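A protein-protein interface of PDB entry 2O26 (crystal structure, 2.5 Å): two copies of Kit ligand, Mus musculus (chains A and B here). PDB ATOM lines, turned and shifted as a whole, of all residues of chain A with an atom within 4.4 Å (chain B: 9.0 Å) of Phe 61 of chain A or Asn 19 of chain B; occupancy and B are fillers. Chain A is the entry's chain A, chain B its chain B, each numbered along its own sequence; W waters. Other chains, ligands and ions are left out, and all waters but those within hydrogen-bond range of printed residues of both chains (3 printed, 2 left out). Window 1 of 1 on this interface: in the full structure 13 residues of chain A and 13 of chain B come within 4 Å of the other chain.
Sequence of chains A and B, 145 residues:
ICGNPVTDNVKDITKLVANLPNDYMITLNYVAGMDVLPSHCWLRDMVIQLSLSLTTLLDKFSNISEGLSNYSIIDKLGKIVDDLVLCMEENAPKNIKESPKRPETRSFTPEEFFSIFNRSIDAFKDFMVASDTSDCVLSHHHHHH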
ATOM      1  N   ASN A  19      -4.859   2.106   9.061  1.00  0.00           N
ATOM      2  CA  ASN A  19      -5.858   1.432   8.263  1.00  0.00           C
ATOM      3  C   ASN A  19      -6.350   2.308   7.108  1.00  0.00           C
ATOM      4  O   ASN A  19      -7.340   1.982   6.449  1.00  0.00           O
ATOM      5  CB  ASN A  19      -7.024   1.029   9.153  1.00  0.00           C
ATOM      6  CG  ASN A  19      -7.581  -0.312   8.784  1.00  0.00           C
ATOM      7  OD1 ASN A  19      -6.822  -1.261   8.568  1.00  0.00           O
ATOM      8  ND2 ASN A  19      -8.911  -0.418   8.730  1.00  0.00           N
ATOM      9  N   LEU A  20      -5.663   3.425   6.868  1.00  0.00           N
ATOM     10  CA  LEU A  20      -6.023   4.320   5.763  1.00  0.00           C
ATOM     11  C   LEU A  20      -4.802   4.496   4.858  1.00  0.00           C
ATOM     12  O   LEU A  20      -3.679   4.605   5.340  1.00  0.00           O
ATOM     13  CB  LEU A  20      -6.493   5.679   6.281  1.00  0.00           C
ATOM     14  CG  LEU A  20      -7.878   5.815   6.916  1.00  0.00           C
ATOM     15  CD1 LEU A  20      -8.083   7.218   7.462  1.00  0.00           C
ATOM     16  CD2 LEU A  20      -8.939   5.484   5.875  1.00  0.00           C
ATOM     17  N   LEU A  57     -15.532  13.117   5.353  1.00  0.00           N
ATOM     18  CA  LEU A  57     -14.736  11.901   5.407  1.00  0.00           C
ATOM     19  C   LEU A  57     -15.628  10.676   5.637  1.00  0.00           C
ATOM     20  O   LEU A  57     -15.496   9.656   4.946  1.00  0.00           O
ATOM     21  CB  LEU A  57     -13.718  11.972   6.540  1.00  0.00           C
ATOM     22  CG  LEU A  57     -12.329  11.400   6.262  1.00  0.00           C
ATOM     23  CD1 LEU A  57     -11.726  10.948   7.578  1.00  0.00           C
ATOM     24  CD2 LEU A  57     -12.381  10.263   5.292  1.00  0.00           C
ATOM     25  N   LEU A  58     -16.527  10.779   6.614  1.00  0.00           N
ATOM     26  CA  LEU A  58     -17.405   9.672   6.946  1.00  0.00           C
ATOM     27  C   LEU A  58     -18.236   9.228   5.764  1.00  0.00           C
ATOM     28  O   LEU A  58     -18.576   8.064   5.645  1.00  0.00           O
ATOM     29  CB  LEU A  58     -18.319  10.051   8.106  1.00  0.00           C
ATOM     30  CG  LEU A  58     -19.119   8.854   8.596  1.00  0.00           C
ATOM     31  CD1 LEU A  58     -18.170   7.786   9.086  1.00  0.00           C
ATOM     32  CD2 LEU A  58     -20.065   9.274   9.689  1.00  0.00           C
ATOM     33  N   ASP A  59     -18.561  10.165   4.885  1.00  0.00           N
ATOM     34  CA  ASP A  59     -19.400   9.879   3.724  1.00  0.00           C
ATOM     35  C   ASP A  59     -18.733   8.872   2.789  1.00  0.00           C
ATOM     36  O   ASP A  59     -19.396   8.201   2.000  1.00  0.00           O
ATOM     37  CB  ASP A  59     -19.694  11.193   2.999  1.00  0.00           C
ATOM     38  CG  ASP A  59     -20.556  11.008   1.785  1.00  0.00           C
ATOM     39  OD1 ASP A  59     -20.365  11.757   0.801  1.00  0.00           O
ATOM     40  OD2 ASP A  59     -21.422  10.110   1.810  1.00  0.00           O
ATOM     41  N   LYS A  60     -17.416   8.751   2.911  1.00  0.00           N
ATOM     42  CA  LYS A  60     -16.621   7.855   2.073  1.00  0.00           C
ATOM     43  C   LYS A  60     -16.581   6.406   2.510  1.00  0.00           C
ATOM     44  O   LYS A  60     -15.993   5.572   1.826  1.00  0.00           O
ATOM     45  CB  LYS A  60     -15.187   8.381   1.999  1.00  0.00           C
ATOM     46  CG  LYS A  60     -14.962   9.436   0.923  1.00  0.00           C
ATOM     47  CD  LYS A  60     -16.086  10.439   0.875  1.00  0.00           C
ATOM     48  CE  LYS A  60     -15.836  11.508  -0.185  1.00  0.00           C
ATOM     49  NZ  LYS A  60     -14.607  12.284   0.115  1.00  0.00           N
ATOM     50  N   PHE A  61     -17.195   6.108   3.652  1.00  0.00           N
ATOM     51  CA  PHE A  61     -17.213   4.749   4.191  1.00  0.00           C
ATOM     52  C   PHE A  61     -18.615   4.217   4.431  1.00  0.00           C
ATOM     53  O   PHE A  61     -19.595   4.971   4.405  1.00  0.00           O
ATOM     54  CB  PHE A  61     -16.409   4.679   5.487  1.00  0.00           C
ATOM     55  CG  PHE A  61     -14.998   5.128   5.339  1.00  0.00           C
ATOM     56  CD1 PHE A  61     -14.676   6.465   5.460  1.00  0.00           C
ATOM     57  CD2 PHE A  61     -13.992   4.216   5.032  1.00  0.00           C
ATOM     58  CE1 PHE A  61     -13.364   6.901   5.272  1.00  0.00           C
ATOM     59  CE2 PHE A  61     -12.680   4.634   4.840  1.00  0.00           C
ATOM     60  CZ  PHE A  61     -12.363   5.985   4.957  1.00  0.00           C
ATOM     61  N   SER A  62     -18.694   2.913   4.685  1.00  0.00           N
ATOM     62  CA  SER A  62     -19.967   2.235   4.943  1.00  0.00           C
ATOM     63  C   SER A  62     -19.869   1.504   6.277  1.00  0.00           C
ATOM     64  O   SER A  62     -18.788   1.044   6.660  1.00  0.00           O
ATOM     65  CB  SER A  62     -20.283   1.210   3.845  1.00  0.00           C
ATOM     66  OG  SER A  62     -20.535   1.832   2.594  1.00  0.00           O
ATOM     67  N   SER A  69     -14.307  -0.558  12.606  1.00  0.00           N
ATOM     68  CA  SER A  69     -14.157  -0.182  11.215  1.00  0.00           C
ATOM     69  C   SER A  69     -13.737   1.277  11.136  1.00  0.00           C
ATOM     70  O   SER A  69     -13.845   2.016  12.115  1.00  0.00           O
ATOM     71  CB  SER A  69     -15.497  -0.355  10.497  1.00  0.00           C
ATOM     72  OG  SER A  69     -16.504   0.430  11.121  1.00  0.00           O
ATOM     73  N   ASN A  70     -13.259   1.696   9.972  1.00  0.00           N
ATOM     74  CA  ASN A  70     -12.877   3.081   9.820  1.00  0.00           C
ATOM     75  C   ASN A  70     -14.143   3.937  10.005  1.00  0.00           C
ATOM     76  O   ASN A  70     -14.100   5.005  10.612  1.00  0.00           O
ATOM     77  CB  ASN A  70     -12.237   3.307   8.459  1.00  0.00           C
ATOM     78  CG  ASN A  70     -10.920   2.579   8.318  1.00  0.00           C
ATOM     79  OD1 ASN A  70     -10.331   2.154   9.311  1.00  0.00           O
ATOM     80  ND2 ASN A  70     -10.438   2.449   7.085  1.00  0.00           N
ATOM     81  N   TYR A  71     -15.282   3.456   9.518  1.00  0.00           N
ATOM     82  CA  TYR A  71     -16.509   4.224   9.659  1.00  0.00           C
ATOM     83  C   TYR A  71     -16.755   4.505  11.134  1.00  0.00           C
ATOM     84  O   TYR A  71     -16.990   5.644  11.524  1.00  0.00           O
ATOM     85  CB  TYR A  71     -17.694   3.455   9.092  1.00  0.00           C
ATOM     86  CG  TYR A  71     -19.001   4.221   9.194  1.00  0.00           C
ATOM     87  CD1 TYR A  71     -19.482   4.987   8.120  1.00  0.00           C
ATOM     88  CD2 TYR A  71     -19.739   4.215  10.383  1.00  0.00           C
ATOM     89  CE1 TYR A  71     -20.661   5.722   8.231  1.00  0.00           C
ATOM     90  CE2 TYR A  71     -20.921   4.952  10.507  1.00  0.00           C
ATOM     91  CZ  TYR A  71     -21.377   5.705   9.428  1.00  0.00           C
ATOM     92  OH  TYR A  71     -22.544   6.435   9.556  1.00  0.00           O
ATOM     93  N   ILE A  74     -14.111   7.164  12.664  1.00  0.00           N
ATOM     94  CA  ILE A  74     -14.383   8.480  12.076  1.00  0.00           C
ATOM     95  C   ILE A  74     -15.679   9.076  12.579  1.00  0.00           C
ATOM     96  O   ILE A  74     -15.765  10.272  12.840  1.00  0.00           O
ATOM     97  CB  ILE A  74     -14.435   8.361  10.543  1.00  0.00           C
ATOM     98  CG1 ILE A  74     -13.053   7.979   9.996  1.00  0.00           C
ATOM     99  CG2 ILE A  74     -14.902   9.679   9.944  1.00  0.00           C
ATOM    100  CD1 ILE A  74     -13.047   7.611   8.542  1.00  0.00           C
ATOM    101  N   ASP B  12     -13.378 -11.830   2.615  1.00  0.00           N
ATOM    102  CA  ASP B  12     -13.172 -10.604   3.370  1.00  0.00           C
ATOM    103  C   ASP B  12     -13.184  -9.347   2.505  1.00  0.00           C
ATOM    104  O   ASP B  12     -12.956  -8.241   3.000  1.00  0.00           O
ATOM    105  CB  ASP B  12     -11.858 -10.688   4.148  1.00  0.00           C
ATOM    106  CG  ASP B  12     -11.952 -11.600   5.359  1.00  0.00           C
ATOM    107  OD1 ASP B  12     -12.897 -11.424   6.160  1.00  0.00           O
ATOM    108  OD2 ASP B  12     -11.079 -12.480   5.526  1.00  0.00           O
ATOM    109  N   ILE B  13     -13.454  -9.512   1.215  1.00  0.00           N
ATOM    110  CA  ILE B  13     -13.480  -8.376   0.316  1.00  0.00           C
ATOM    111  C   ILE B  13     -14.590  -7.389   0.673  1.00  0.00           C
ATOM    112  O   ILE B  13     -14.362  -6.185   0.733  1.00  0.00           O
ATOM    113  CB  ILE B  13     -13.622  -8.850  -1.160  1.00  0.00           C
ATOM    114  CG1 ILE B  13     -12.331  -9.567  -1.590  1.00  0.00           C
ATOM    115  CG2 ILE B  13     -13.911  -7.665  -2.078  1.00  0.00           C
ATOM    116  CD1 ILE B  13     -12.357 -10.121  -3.009  1.00  0.00           C
ATOM    117  N   THR B  14     -15.793  -7.886   0.922  1.00  0.00           N
ATOM    118  CA  THR B  14     -16.894  -6.994   1.277  1.00  0.00           C
ATOM    119  C   THR B  14     -16.503  -6.115   2.467  1.00  0.00           C
ATOM    120  O   THR B  14     -16.734  -4.902   2.475  1.00  0.00           O
ATOM    121  CB  THR B  14     -18.138  -7.802   1.616  1.00  0.00           C
ATOM    122  OG1 THR B  14     -18.429  -8.682   0.526  1.00  0.00           O
ATOM    123  CG2 THR B  14     -19.315  -6.890   1.858  1.00  0.00           C
ATOM    124  N   LYS B  15     -15.897  -6.726   3.473  1.00  0.00           N
ATOM    125  CA  LYS B  15     -15.470  -5.997   4.660  1.00  0.00           C
ATOM    126  C   LYS B  15     -14.403  -4.976   4.255  1.00  0.00           C
ATOM    127  O   LYS B  15     -14.488  -3.801   4.602  1.00  0.00           O
ATOM    128  CB  LYS B  15     -14.892  -6.980   5.682  1.00  0.00           C
ATOM    129  CG  LYS B  15     -14.447  -6.358   6.987  1.00  0.00           C
ATOM    130  CD  LYS B  15     -13.963  -7.423   7.964  1.00  0.00           C
ATOM    131  CE  LYS B  15     -13.667  -6.839   9.352  1.00  0.00           C
ATOM    132  NZ  LYS B  15     -12.594  -5.793   9.352  1.00  0.00           N
ATOM    133  N   LEU B  16     -13.412  -5.429   3.495  1.00  0.00           N
ATOM    134  CA  LEU B  16     -12.322  -4.567   3.036  1.00  0.00           C
ATOM    135  C   LEU B  16     -12.836  -3.322   2.299  1.00  0.00           C
ATOM    136  O   LEU B  16     -12.452  -2.188   2.604  1.00  0.00           O
ATOM    137  CB  LEU B  16     -11.390  -5.374   2.119  1.00  0.00           C
ATOM    138  CG  LEU B  16      -9.974  -4.892   1.745  1.00  0.00           C
ATOM    139  CD1 LEU B  16      -9.894  -4.699   0.236  1.00  0.00           C
ATOM    140  CD2 LEU B  16      -9.623  -3.604   2.463  1.00  0.00           C
ATOM    141  N   VAL B  17     -13.713  -3.538   1.326  1.00  0.00           N
ATOM    142  CA  VAL B  17     -14.260  -2.440   0.556  1.00  0.00           C
ATOM    143  C   VAL B  17     -14.972  -1.437   1.448  1.00  0.00           C
ATOM    144  O   VAL B  17     -14.772  -0.223   1.323  1.00  0.00           O
ATOM    145  CB  VAL B  17     -15.229  -2.947  -0.524  1.00  0.00           C
ATOM    146  CG1 VAL B  17     -16.016  -1.777  -1.110  1.00  0.00           C
ATOM    147  CG2 VAL B  17     -14.434  -3.638  -1.633  1.00  0.00           C
ATOM    148  N   ALA B  18     -15.805  -1.935   2.356  1.00  0.00           N
ATOM    149  CA  ALA B  18     -16.541  -1.045   3.261  1.00  0.00           C
ATOM    150  C   ALA B  18     -15.560  -0.281   4.169  1.00  0.00           C
ATOM    151  O   ALA B  18     -15.897   0.751   4.768  1.00  0.00           O
ATOM    152  CB  ALA B  18     -17.497  -1.870   4.121  1.00  0.00           C
ATOM    153  N   ASN B  19     -14.330  -0.779   4.247  1.00  0.00           N
ATOM    154  CA  ASN B  19     -13.333  -0.154   5.099  1.00  0.00           C
ATOM    155  C   ASN B  19     -12.335   0.673   4.301  1.00  0.00           C
ATOM    156  O   ASN B  19     -11.294   1.065   4.814  1.00  0.00           O
ATOM    157  CB  ASN B  19     -12.608  -1.228   5.903  1.00  0.00           C
ATOM    158  CG  ASN B  19     -12.335  -0.803   7.315  1.00  0.00           C
ATOM    159  OD1 ASN B  19     -13.207  -0.257   7.990  1.00  0.00           O
ATOM    160  ND2 ASN B  19     -11.121  -1.061   7.785  1.00  0.00           N
ATOM    161  N   LEU B  20     -12.637   0.906   3.027  1.00  0.00           N
ATOM    162  CA  LEU B  20     -11.796   1.754   2.174  1.00  0.00           C
ATOM    163  C   LEU B  20     -12.652   2.893   1.608  1.00  0.00           C
ATOM    164  O   LEU B  20     -13.813   2.689   1.251  1.00  0.00           O
ATOM    165  CB  LEU B  20     -11.193   0.939   1.041  1.00  0.00           C
ATOM    166  CG  LEU B  20     -10.049  -0.028   1.356  1.00  0.00           C
ATOM    167  CD1 LEU B  20      -9.658  -0.811   0.117  1.00  0.00           C
ATOM    168  CD2 LEU B  20      -8.868   0.743   1.891  1.00  0.00           C
ATOM    169  N   PRO B  21     -12.076   4.098   1.498  1.00  0.00           N
ATOM    170  CA  PRO B  21     -12.796   5.263   0.979  1.00  0.00           C
ATOM    171  C   PRO B  21     -13.359   4.971  -0.399  1.00  0.00           C
ATOM    172  O   PRO B  21     -12.629   4.521  -1.266  1.00  0.00           O
ATOM    173  CB  PRO B  21     -11.725   6.346   0.939  1.00  0.00           C
ATOM    174  CG  PRO B  21     -10.705   5.899   1.937  1.00  0.00           C
ATOM    175  CD  PRO B  21     -10.653   4.421   1.691  1.00  0.00           C
ATOM    176  N   ASN B  22     -14.644   5.241  -0.605  1.00  0.00           N
ATOM    177  CA  ASN B  22     -15.268   4.937  -1.887  1.00  0.00           C
ATOM    178  C   ASN B  22     -14.822   5.846  -3.021  1.00  0.00           C
ATOM    179  O   ASN B  22     -15.201   5.647  -4.174  1.00  0.00           O
ATOM    180  CB  ASN B  22     -16.800   4.978  -1.751  1.00  0.00           C
ATOM    181  CG  ASN B  22     -17.278   6.144  -0.960  1.00  0.00           C
ATOM    182  OD1 ASN B  22     -16.866   7.280  -1.192  1.00  0.00           O
ATOM    183  ND2 ASN B  22     -18.178   5.883  -0.009  1.00  0.00           N
ATOM    184  N   ASP B  23     -14.010   6.840  -2.689  1.00  0.00           N
ATOM    185  CA  ASP B  23     -13.523   7.786  -3.683  1.00  0.00           C
ATOM    186  C   ASP B  23     -12.012   7.663  -3.811  1.00  0.00           C
ATOM    187  O   ASP B  23     -11.353   8.534  -4.368  1.00  0.00           O
ATOM    188  CB  ASP B  23     -13.914   9.205  -3.265  1.00  0.00           C
ATOM    189  CG  ASP B  23     -13.229   9.648  -1.981  1.00  0.00           C
ATOM    190  OD1 ASP B  23     -12.854   8.784  -1.165  1.00  0.00           O
ATOM    191  OD2 ASP B  23     -13.071  10.869  -1.773  1.00  0.00           O
ATOM    192  N   TYR B  24     -11.460   6.579  -3.285  1.00  0.00           N
ATOM    193  CA  TYR B  24     -10.021   6.349  -3.352  1.00  0.00           C
ATOM    194  C   TYR B  24      -9.759   5.591  -4.628  1.00  0.00           C
ATOM    195  O   TYR B  24     -10.322   4.520  -4.837  1.00  0.00           O
ATOM    196  CB  TYR B  24      -9.567   5.495  -2.166  1.00  0.00           C
ATOM    197  CG  TYR B  24      -8.095   5.176  -2.167  1.00  0.00           C
ATOM    198  CD1 TYR B  24      -7.143   6.191  -2.061  1.00  0.00           C
ATOM    199  CD2 TYR B  24      -7.645   3.858  -2.281  1.00  0.00           C
ATOM    200  CE1 TYR B  24      -5.753   5.890  -2.064  1.00  0.00           C
ATOM    201  CE2 TYR B  24      -6.268   3.548  -2.285  1.00  0.00           C
ATOM    202  CZ  TYR B  24      -5.333   4.573  -2.178  1.00  0.00           C
ATOM    203  OH  TYR B  24      -3.993   4.306  -2.172  1.00  0.00           O
ATOM    204  N   PHE B  61      -0.403   0.776   3.385  1.00  0.00           N
ATOM    205  CA  PHE B  61      -0.866   0.463   4.728  1.00  0.00           C
ATOM    206  C   PHE B  61       0.236  -0.041   5.636  1.00  0.00           C
ATOM    207  O   PHE B  61       1.333  -0.391   5.185  1.00  0.00           O
ATOM    208  CB  PHE B  61      -1.993  -0.567   4.682  1.00  0.00           C
ATOM    209  CG  PHE B  61      -3.157  -0.140   3.840  1.00  0.00           C
ATOM    210  CD1 PHE B  61      -3.182  -0.401   2.473  1.00  0.00           C
ATOM    211  CD2 PHE B  61      -4.215   0.556   4.404  1.00  0.00           C
ATOM    212  CE1 PHE B  61      -4.252   0.026   1.679  1.00  0.00           C
ATOM    213  CE2 PHE B  61      -5.293   0.990   3.623  1.00  0.00           C
ATOM    214  CZ  PHE B  61      -5.310   0.723   2.249  1.00  0.00           C
ATOM    215  N   GLY B  67      -6.402  -7.833  14.897  1.00  0.00           N
ATOM    216  CA  GLY B  67      -7.643  -7.482  14.229  1.00  0.00           C
ATOM    217  C   GLY B  67      -7.532  -7.356  12.721  1.00  0.00           C
ATOM    218  O   GLY B  67      -6.568  -6.789  12.207  1.00  0.00           O
ATOM    219  N   LEU B  68      -8.524  -7.893  12.012  1.00  0.00           N
ATOM    220  CA  LEU B  68      -8.544  -7.840  10.554  1.00  0.00           C
ATOM    221  C   LEU B  68      -8.402  -6.417  10.026  1.00  0.00           C
ATOM    222  O   LEU B  68      -9.370  -5.663   9.901  1.00  0.00           O
ATOM    223  CB  LEU B  68      -9.828  -8.464  10.005  1.00  0.00           C
ATOM    224  CG  LEU B  68      -9.753  -9.951   9.656  1.00  0.00           C
ATOM    225  CD1 LEU B  68     -11.099 -10.426   9.127  1.00  0.00           C
ATOM    226  CD2 LEU B  68      -8.659 -10.172   8.614  1.00  0.00           C
ATOM    227  N   SER B  69      -7.164  -6.062   9.723  1.00  0.00           N
ATOM    228  CA  SER B  69      -6.847  -4.753   9.213  1.00  0.00           C
ATOM    229  C   SER B  69      -6.865  -4.810   7.693  1.00  0.00           C
ATOM    230  O   SER B  69      -6.876  -5.885   7.108  1.00  0.00           O
ATOM    231  CB  SER B  69      -5.446  -4.358   9.681  1.00  0.00           C
ATOM    232  OG  SER B  69      -4.484  -5.320   9.278  1.00  0.00           O
ATOM    233  N   ASN B  70      -6.878  -3.649   7.055  1.00  0.00           N
ATOM    234  CA  ASN B  70      -6.855  -3.609   5.611  1.00  0.00           C
ATOM    235  C   ASN B  70      -5.536  -4.226   5.138  1.00  0.00           C
ATOM    236  O   ASN B  70      -5.492  -4.936   4.143  1.00  0.00           O
ATOM    237  CB  ASN B  70      -7.025  -2.183   5.101  1.00  0.00           C
ATOM    238  CG  ASN B  70      -8.410  -1.622   5.397  1.00  0.00           C
ATOM    239  OD1 ASN B  70      -9.340  -2.367   5.704  1.00  0.00           O
ATOM    240  ND2 ASN B  70      -8.554  -0.312   5.293  1.00  0.00           N
ATOM    241  N   TYR B  71      -4.457  -3.983   5.870  1.00  0.00           N
ATOM    242  CA  TYR B  71      -3.167  -4.532   5.482  1.00  0.00           C
ATOM    243  C   TYR B  71      -3.268  -6.050   5.408  1.00  0.00           C
ATOM    244  O   TYR B  71      -2.858  -6.667   4.432  1.00  0.00           O
ATOM    245  CB  TYR B  71      -2.097  -4.151   6.496  1.00  0.00           C
ATOM    246  CG  TYR B  71      -0.716  -4.681   6.150  1.00  0.00           C
ATOM    247  CD1 TYR B  71       0.202  -3.895   5.460  1.00  0.00           C
ATOM    248  CD2 TYR B  71      -0.350  -5.993   6.457  1.00  0.00           C
ATOM    249  CE1 TYR B  71       1.443  -4.408   5.077  1.00  0.00           C
ATOM    250  CE2 TYR B  71       0.879  -6.507   6.074  1.00  0.00           C
ATOM    251  CZ  TYR B  71       1.780  -5.717   5.383  1.00  0.00           C
ATOM    252  OH  TYR B  71       3.002  -6.245   4.994  1.00  0.00           O
ATOM    253  N   ILE B  73      -5.900  -8.182   5.041  1.00  0.00           N
ATOM    254  CA  ILE B  73      -6.666  -8.648   3.892  1.00  0.00           C
ATOM    255  C   ILE B  73      -5.893  -8.507   2.581  1.00  0.00           C
ATOM    256  O   ILE B  73      -5.654  -9.494   1.875  1.00  0.00           O
ATOM    257  CB  ILE B  73      -7.986  -7.871   3.728  1.00  0.00           C
ATOM    258  CG1 ILE B  73      -8.720  -7.738   5.070  1.00  0.00           C
ATOM    259  CG2 ILE B  73      -8.841  -8.561   2.673  1.00  0.00           C
ATOM    260  CD1 ILE B  73      -9.451  -8.972   5.519  1.00  0.00           C
ATOM    261  N   ILE B  74      -5.521  -7.267   2.256  1.00  0.00           N
ATOM    262  CA  ILE B  74      -4.784  -6.969   1.030  1.00  0.00           C
ATOM    263  C   ILE B  74      -3.577  -7.871   0.861  1.00  0.00           C
ATOM    264  O   ILE B  74      -3.285  -8.342  -0.232  1.00  0.00           O
ATOM    265  CB  ILE B  74      -4.343  -5.497   1.016  1.00  0.00           C
ATOM    266  CG1 ILE B  74      -5.582  -4.590   0.969  1.00  0.00           C
ATOM    267  CG2 ILE B  74      -3.413  -5.247  -0.156  1.00  0.00           C
ATOM    268  CD1 ILE B  74      -5.271  -3.120   1.201  1.00  0.00           C
ATOM    269  N   PRO B 110     -12.368   1.273  -4.919  1.00  0.00           N
ATOM    270  CA  PRO B 110     -12.179  -0.055  -4.324  1.00  0.00           C
ATOM    271  C   PRO B 110     -13.266  -1.012  -4.828  1.00  0.00           C
ATOM    272  O   PRO B 110     -12.959  -2.108  -5.291  1.00  0.00           O
ATOM    273  CB  PRO B 110     -12.295   0.231  -2.827  1.00  0.00           C
ATOM    274  CG  PRO B 110     -11.648   1.592  -2.720  1.00  0.00           C
ATOM    275  CD  PRO B 110     -12.260   2.338  -3.905  1.00  0.00           C
HETATM  276  O   HOH W   1      -4.241  -2.121   8.216  1.00  0.00           O
HETATM  277  O   HOH W   2      -8.906  -2.694  11.371  1.00  0.00           O
HETATM  278  O   HOH W   3     -18.818   3.216   0.465  1.00  0.00           O
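The backbone carbonyl oxygen (O) of Lys 60 of chain A is in hydrogen-bond range of the backbone NH (N) of Asn 22 of chain B, 2.8 Å away. N of Asn 70 of chain A is in hydrogen-bond range of OD1 of Asn 19 of chain B (2.8 Å). The side-chain amide oxygen (OD1) of Asn 19 of chain A is in hydrogen-bond range of the backbone NH (N) of Asn 70 of chain B (2.8 Å). The backbone carbonyl oxygen of Asp 59 of chain A sits at hydrogen-bond distance from the side-chain amide nitrogen of Asn 22 of chain B (3.3 Å). O of Ser 62 of chain A sits close to O of Ala 18 of chain B. The side-chain amino group (NZ) of Lys 60 of chain A is in salt-bridge range of the side-chain carboxylate (OD2) of Asp 23 of chain B, 2.8 Å away. ND2 of Asn 19 of chain B sits close to ND2 of Asn 19 of chain A (2.5 Å).
The side-chain amide oxygen of Asn 70 of chain B is in hydrogen-bond range of the side-chain amide nitrogen of Asn 19 of chain B, 3.0 Å away. The side-chain amide nitrogen of Asn 19 of chain A is in hydrogen-bond range of the side-chain amide oxygen of Asn 70 of chain A, at 3.0 Å.
Of chain A, only Asn 19, Phe 61, Ser 69 and Asn 70 come within 4 Å of Asn 19 of chain B. Ser 69 of chain A touches just one residue of chain B: Asn 19 (3.4 Å). Printed residues of chain B within 4 Å of Asn 70 of chain A: Asn 19 (2.8 Å) and Asn 70 (3.8 Å). Printed residues of chain A within 4 Å of Leu 20 of chain B: Lys 60 (3.7 Å) and Phe 61 (3.7 Å). The nearest printed residue of chain A that does not touch Asn 19 of chain B is Tyr 71 of chain A (4.5 Å). The nearest printed residue of chain B that does not touch Asn 70 of chain A is Leu 20 of chain B (4.9 Å).
Water W1 lies within hydrogen-bond range of OD1 of Asn 19 of chain A (2.7 Å), N of Tyr 71 of chain B (3.0 Å), N of Asn 70 of chain B (3.3 Å) and OG of Ser 69 of chain B (3.4 Å). Water W3 lies within hydrogen-bond range of the side-chain amide nitrogen (ND2) of Asn 22 of chain B (2.8 Å) and the side-chain hydroxyl (OG) of Ser 62 of chain A (3.1 Å). Water W2 bridges O of Leu 68 of chain B (3.3 Å) and ND2 of Asn 19 of chain A (3.5 Å).
Hydrophobic or aromatic side chains of chain B that line the printed part of chain A: Pro 21 and Phe 61. Among the printed residues, 19 pairs touch across the chains.
Among the printed residues, merely in contact across the chains: Asn 19 of chain A with Phe 61 of chain B (3.6 Å), Asn 19 of chain A with Ser 69 of chain B (3.6 Å), Leu 20 of chain A with Phe 61 of chain B (3.7 Å), Lys 60 of chain A with Leu 20 of chain B (3.7 Å), Lys 60 of chain A with Pro 21 of chain B (3.3 Å), Phe 61 of chain A with Ala 18 of chain B (3.96 Å), Phe 61 of chain A with Asn 19 of chain B (3.8 Å), Phe 61 of chain A with Leu 20 of chain B (3.7 Å), Phe 61 of chain A with Pro 21 of chain B (3.4 Å), Phe 61 of chain A with Asn 22 of chain B (3.8 Å), Ser 69 of chain A with Asn 19 of chain B (3.4 Å) and Asn 70 of chain A with Asn 70 of chain B (3.8 Å).
Asn 19 of chain A touches its own counterpart, Asn 19 of chain B. Asn 19 of chain A touches Phe 61 of chain B, and with the chains exchanged Phe 61 of chain A touches Asn 19 of chain B. Asn 19 of chain A touches Ser 69 of chain B, and with the chains exchanged Ser 69 of chain A touches Asn 19 of chain B. Asn 70 of chain A touches its own counterpart, Asn 70 of chain B. Positions printed for both chains: 19, 20, 61, 69, 70, 71 and 74. Of the 19 pairs that touch across the chains among the printed residues, 10 have their exchanged pair printed and touching as well.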
